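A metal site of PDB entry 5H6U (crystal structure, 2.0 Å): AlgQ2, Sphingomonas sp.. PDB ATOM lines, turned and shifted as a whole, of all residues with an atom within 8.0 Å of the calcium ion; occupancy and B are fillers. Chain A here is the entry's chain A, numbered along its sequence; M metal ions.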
ATOM      1  N   TRP A 145      -1.745 -28.615  16.587  1.00  0.00           N
ATOM      2  CA  TRP A 145      -2.644 -27.565  17.061  1.00  0.00           C
ATOM      3  C   TRP A 145      -4.095 -28.061  17.071  1.00  0.00           C
ATOM      4  O   TRP A 145      -4.840 -27.761  17.999  1.00  0.00           O
ATOM      5  CB  TRP A 145      -2.514 -26.304  16.210  1.00  0.00           C
ATOM      6  CG  TRP A 145      -1.281 -25.564  16.473  1.00  0.00           C
ATOM      7  CD1 TRP A 145      -0.257 -25.941  17.294  1.00  0.00           C
ATOM      8  CD2 TRP A 145      -0.890 -24.310  15.896  1.00  0.00           C
ATOM      9  NE1 TRP A 145       0.736 -24.989  17.276  1.00  0.00           N
ATOM     10  CE2 TRP A 145       0.361 -23.977  16.436  1.00  0.00           C
ATOM     11  CE3 TRP A 145      -1.514 -23.423  14.999  1.00  0.00           C
ATOM     12  CZ2 TRP A 145       1.034 -22.805  16.087  1.00  0.00           C
ATOM     13  CZ3 TRP A 145      -0.832 -22.242  14.654  1.00  0.00           C
ATOM     14  CH2 TRP A 145       0.424 -21.946  15.197  1.00  0.00           C
ATOM     15  N   PHE A 167      -7.138 -21.175  15.396  1.00  0.00           N
ATOM     16  CA  PHE A 167      -5.684 -20.977  15.477  1.00  0.00           C
ATOM     17  C   PHE A 167      -5.381 -19.557  15.883  1.00  0.00           C
ATOM     18  O   PHE A 167      -4.509 -19.310  16.740  1.00  0.00           O
ATOM     19  CB  PHE A 167      -5.017 -21.283  14.142  1.00  0.00           C
ATOM     20  CG  PHE A 167      -4.937 -22.728  13.810  1.00  0.00           C
ATOM     21  CD1 PHE A 167      -5.308 -23.679  14.734  1.00  0.00           C
ATOM     22  CD2 PHE A 167      -4.530 -23.144  12.547  1.00  0.00           C
ATOM     23  CE1 PHE A 167      -5.242 -25.023  14.438  1.00  0.00           C
ATOM     24  CE2 PHE A 167      -4.463 -24.502  12.211  1.00  0.00           C
ATOM     25  CZ  PHE A 167      -4.818 -25.438  13.161  1.00  0.00           C
ATOM     26  N   LYS A 168      -6.122 -18.613  15.295  1.00  0.00           N
ATOM     27  CA  LYS A 168      -5.896 -17.197  15.533  1.00  0.00           C
ATOM     28  C   LYS A 168      -6.218 -16.827  16.964  1.00  0.00           C
ATOM     29  O   LYS A 168      -5.419 -16.171  17.637  1.00  0.00           O
ATOM     30  CB  LYS A 168      -6.746 -16.381  14.572  1.00  0.00           C
ATOM     31  CG  LYS A 168      -6.485 -14.893  14.624  1.00  0.00           C
ATOM     32  CD  LYS A 168      -5.146 -14.541  13.987  1.00  0.00           C
ATOM     33  CE  LYS A 168      -4.963 -13.042  13.911  1.00  0.00           C
ATOM     34  NZ  LYS A 168      -4.947 -12.450  15.315  1.00  0.00           N
ATOM     35  N   GLU A 169      -7.399 -17.234  17.452  1.00  0.00           N
ATOM     36  CA  GLU A 169      -7.994 -16.666  18.652  1.00  0.00           C
ATOM     37  C   GLU A 169      -7.742 -17.453  19.924  1.00  0.00           C
ATOM     38  O   GLU A 169      -7.915 -16.905  21.013  1.00  0.00           O
ATOM     39  CB  GLU A 169      -9.506 -16.535  18.461  1.00  0.00           C
ATOM     40  CG  GLU A 169      -9.914 -15.646  17.301  1.00  0.00           C
ATOM     41  CD  GLU A 169     -11.415 -15.514  17.197  1.00  0.00           C
ATOM     42  OE1 GLU A 169     -11.865 -14.468  16.693  1.00  0.00           O
ATOM     43  OE2 GLU A 169     -12.141 -16.440  17.628  1.00  0.00           O
ATOM     44  N   LYS A 170      -7.343 -18.707  19.833  1.00  0.00           N
ATOM     45  CA  LYS A 170      -7.286 -19.532  21.039  1.00  0.00           C
ATOM     46  C   LYS A 170      -5.893 -20.095  21.310  1.00  0.00           C
ATOM     47  O   LYS A 170      -5.765 -21.221  21.791  1.00  0.00           O
ATOM     48  CB  LYS A 170      -8.315 -20.651  20.975  1.00  0.00           C
ATOM     49  CG  LYS A 170      -9.735 -20.188  21.317  1.00  0.00           C
ATOM     50  CD  LYS A 170     -10.410 -21.135  22.317  1.00  0.00           C
ATOM     51  CE  LYS A 170      -9.769 -21.041  23.708  1.00  0.00           C
ATOM     52  NZ  LYS A 170     -10.002 -19.731  24.388  1.00  0.00           N
ATOM     53  N   ASP A 171      -4.854 -19.317  21.004  1.00  0.00           N
ATOM     54  CA  ASP A 171      -3.500 -19.535  21.518  1.00  0.00           C
ATOM     55  C   ASP A 171      -2.988 -20.975  21.472  1.00  0.00           C
ATOM     56  O   ASP A 171      -2.507 -21.494  22.490  1.00  0.00           O
ATOM     57  CB  ASP A 171      -3.452 -19.005  22.942  1.00  0.00           C
ATOM     58  CG  ASP A 171      -2.046 -18.937  23.496  1.00  0.00           C
ATOM     59  OD1 ASP A 171      -1.145 -18.571  22.723  1.00  0.00           O
ATOM     60  OD2 ASP A 171      -1.845 -19.274  24.679  1.00  0.00           O
ATOM     61  N   PRO A 172      -3.046 -21.642  20.319  1.00  0.00           N
ATOM     62  CA  PRO A 172      -2.569 -23.042  20.282  1.00  0.00           C
ATOM     63  C   PRO A 172      -1.103 -23.226  20.621  1.00  0.00           C
ATOM     64  O   PRO A 172      -0.732 -24.326  21.047  1.00  0.00           O
ATOM     65  CB  PRO A 172      -2.886 -23.485  18.841  1.00  0.00           C
ATOM     66  CG  PRO A 172      -3.104 -22.220  18.070  1.00  0.00           C
ATOM     67  CD  PRO A 172      -3.680 -21.253  19.047  1.00  0.00           C
ATOM     68  N   ASN A 173      -0.243 -22.213  20.441  1.00  0.00           N
ATOM     69  CA  ASN A 173       1.119 -22.437  20.882  1.00  0.00           C
ATOM     70  C   ASN A 173       1.303 -22.235  22.384  1.00  0.00           C
ATOM     71  O   ASN A 173       2.405 -22.516  22.894  1.00  0.00           O
ATOM     72  CB  ASN A 173       2.134 -21.575  20.108  1.00  0.00           C
ATOM     73  CG  ASN A 173       1.951 -20.066  20.273  1.00  0.00           C
ATOM     74  OD1 ASN A 173       1.344 -19.577  21.219  1.00  0.00           O
ATOM     75  ND2 ASN A 173       2.510 -19.307  19.315  1.00  0.00           N
ATOM     76  N   GLY A 174       0.271 -21.788  23.084  1.00  0.00           N
ATOM     77  CA  GLY A 174       0.280 -21.683  24.538  1.00  0.00           C
ATOM     78  C   GLY A 174       1.393 -20.815  25.056  1.00  0.00           C
ATOM     79  O   GLY A 174       2.313 -21.284  25.728  1.00  0.00           O
ATOM     80  N   ASN A 175       1.349 -19.533  24.712  1.00  0.00           N
ATOM     81  CA  ASN A 175       2.247 -18.543  25.270  1.00  0.00           C
ATOM     82  C   ASN A 175       1.471 -17.314  25.683  1.00  0.00           C
ATOM     83  O   ASN A 175       2.057 -16.246  25.878  1.00  0.00           O
ATOM     84  CB  ASN A 175       3.369 -18.193  24.286  1.00  0.00           C
ATOM     85  CG  ASN A 175       2.848 -17.635  22.949  1.00  0.00           C
ATOM     86  OD1 ASN A 175       1.684 -17.232  22.807  1.00  0.00           O
ATOM     87  ND2 ASN A 175       3.738 -17.562  21.973  1.00  0.00           N
ATOM     88  N   GLY A 176       0.149 -17.434  25.783  1.00  0.00           N
ATOM     89  CA  GLY A 176      -0.703 -16.336  26.164  1.00  0.00           C
ATOM     90  C   GLY A 176      -0.872 -15.244  25.142  1.00  0.00           C
ATOM     91  O   GLY A 176      -1.735 -14.379  25.324  1.00  0.00           O
ATOM     92  N   LYS A 177      -0.096 -15.259  24.054  1.00  0.00           N
ATOM     93  CA  LYS A 177      -0.095 -14.177  23.075  1.00  0.00           C
ATOM     94  C   LYS A 177      -0.867 -14.558  21.817  1.00  0.00           C
ATOM     95  O   LYS A 177      -0.854 -15.719  21.397  1.00  0.00           O
ATOM     96  CB  LYS A 177       1.323 -13.778  22.685  1.00  0.00           C
ATOM     97  CG  LYS A 177       2.243 -13.543  23.852  1.00  0.00           C
ATOM     98  CD  LYS A 177       3.570 -12.911  23.405  1.00  0.00           C
ATOM     99  CE  LYS A 177       4.136 -13.551  22.149  1.00  0.00           C
ATOM    100  NZ  LYS A 177       5.426 -12.895  21.749  1.00  0.00           N
ATOM    101  N   ALA A 178      -1.520 -13.568  21.210  1.00  0.00           N
ATOM    102  CA  ALA A 178      -2.184 -13.776  19.935  1.00  0.00           C
ATOM    103  C   ALA A 178      -1.167 -13.510  18.836  1.00  0.00           C
ATOM    104  O   ALA A 178      -1.216 -12.537  18.085  1.00  0.00           O
ATOM    105  CB  ALA A 178      -3.426 -12.902  19.803  1.00  0.00           C
ATOM    106  N   ASP A 179      -0.205 -14.416  18.778  1.00  0.00           N
ATOM    107  CA  ASP A 179       0.845 -14.335  17.780  1.00  0.00           C
ATOM    108  C   ASP A 179       0.626 -15.293  16.627  1.00  0.00           C
ATOM    109  O   ASP A 179       1.391 -15.239  15.665  1.00  0.00           O
ATOM    110  CB  ASP A 179       2.214 -14.606  18.423  1.00  0.00           C
ATOM    111  CG  ASP A 179       2.274 -15.932  19.142  1.00  0.00           C
ATOM    112  OD1 ASP A 179       1.198 -16.469  19.505  1.00  0.00           O
ATOM    113  OD2 ASP A 179       3.404 -16.423  19.368  1.00  0.00           O
ATOM    114  N   GLU A 180      -0.379 -16.179  16.709  1.00  0.00           N
ATOM    115  CA  GLU A 180      -0.588 -17.199  15.693  1.00  0.00           C
ATOM    116  C   GLU A 180      -1.002 -16.567  14.378  1.00  0.00           C
ATOM    117  O   GLU A 180      -1.878 -15.689  14.336  1.00  0.00           O
ATOM    118  CB  GLU A 180      -1.665 -18.202  16.113  1.00  0.00           C
ATOM    119  CG  GLU A 180      -1.173 -19.285  17.036  1.00  0.00           C
ATOM    120  CD  GLU A 180      -1.035 -18.822  18.478  1.00  0.00           C
ATOM    121  OE1 GLU A 180      -0.740 -19.698  19.309  1.00  0.00           O
ATOM    122  OE2 GLU A 180      -1.201 -17.600  18.776  1.00  0.00           O
ATOM    123  N   VAL A 181      -0.452 -17.083  13.293  1.00  0.00           N
ATOM    124  CA  VAL A 181      -0.759 -16.638  11.948  1.00  0.00           C
ATOM    125  C   VAL A 181      -1.292 -17.829  11.157  1.00  0.00           C
ATOM    126  O   VAL A 181      -0.535 -18.653  10.661  1.00  0.00           O
ATOM    127  CB  VAL A 181       0.478 -16.025  11.283  1.00  0.00           C
ATOM    128  CG1 VAL A 181       0.172 -15.621   9.842  1.00  0.00           C
ATOM    129  CG2 VAL A 181       0.953 -14.858  12.135  1.00  0.00           C
ATOM    130  N   ASN A 262       6.902 -21.339  15.183  1.00  0.00           N
ATOM    131  CA  ASN A 262       5.664 -21.859  15.764  1.00  0.00           C
ATOM    132  C   ASN A 262       4.538 -20.815  15.717  1.00  0.00           C
ATOM    133  O   ASN A 262       3.746 -20.683  16.652  1.00  0.00           O
ATOM    134  CB  ASN A 262       5.906 -22.342  17.195  1.00  0.00           C
ATOM    135  CG  ASN A 262       4.839 -23.326  17.689  1.00  0.00           C
ATOM    136  OD1 ASN A 262       4.093 -23.942  16.903  1.00  0.00           O
ATOM    137  ND2 ASN A 262       4.774 -23.471  19.000  1.00  0.00           N
ATOM    138  N   LEU A 263       4.445 -20.115  14.586  1.00  0.00           N
ATOM    139  CA  LEU A 263       3.396 -19.123  14.395  1.00  0.00           C
ATOM    140  C   LEU A 263       2.354 -19.529  13.359  1.00  0.00           C
ATOM    141  O   LEU A 263       1.209 -19.069  13.437  1.00  0.00           O
ATOM    142  CB  LEU A 263       4.006 -17.787  13.962  1.00  0.00           C
ATOM    143  CG  LEU A 263       5.077 -17.214  14.891  1.00  0.00           C
ATOM    144  CD1 LEU A 263       5.614 -15.895  14.287  1.00  0.00           C
ATOM    145  CD2 LEU A 263       4.460 -17.011  16.250  1.00  0.00           C
HETATM  146 CA    CA M   1       0.041 -17.785  20.976  1.00  0.00          CA
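N of Gly 176 lies within hydrogen-bond range of OD2 of Asp 171, at 2.9 Å. ND2 of Asn 173 sits at hydrogen-bond distance from O of Asn 262 (3.2 Å).
Within 4 Å of the calcium ion: Asp 171, Asn 173, Asn 175, Lys 177, Asp 179 and Glu 180.
The calcium ion is bound by the side-chain amide oxygen (OD1) of Asn 173, the side-chain carboxylate (OD1) of Asp 171, the side-chain carboxylate (OD1) of Asp 179, the backbone carbonyl oxygen (O) of Lys 177, the side-chain amide oxygen (OD1) of Asn 175, the side-chain carboxylate (OE2) of Glu 180 and the side-chain carboxylate (OE1) of Glu 180. The calcium ion has seven donor atoms within binding distance.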
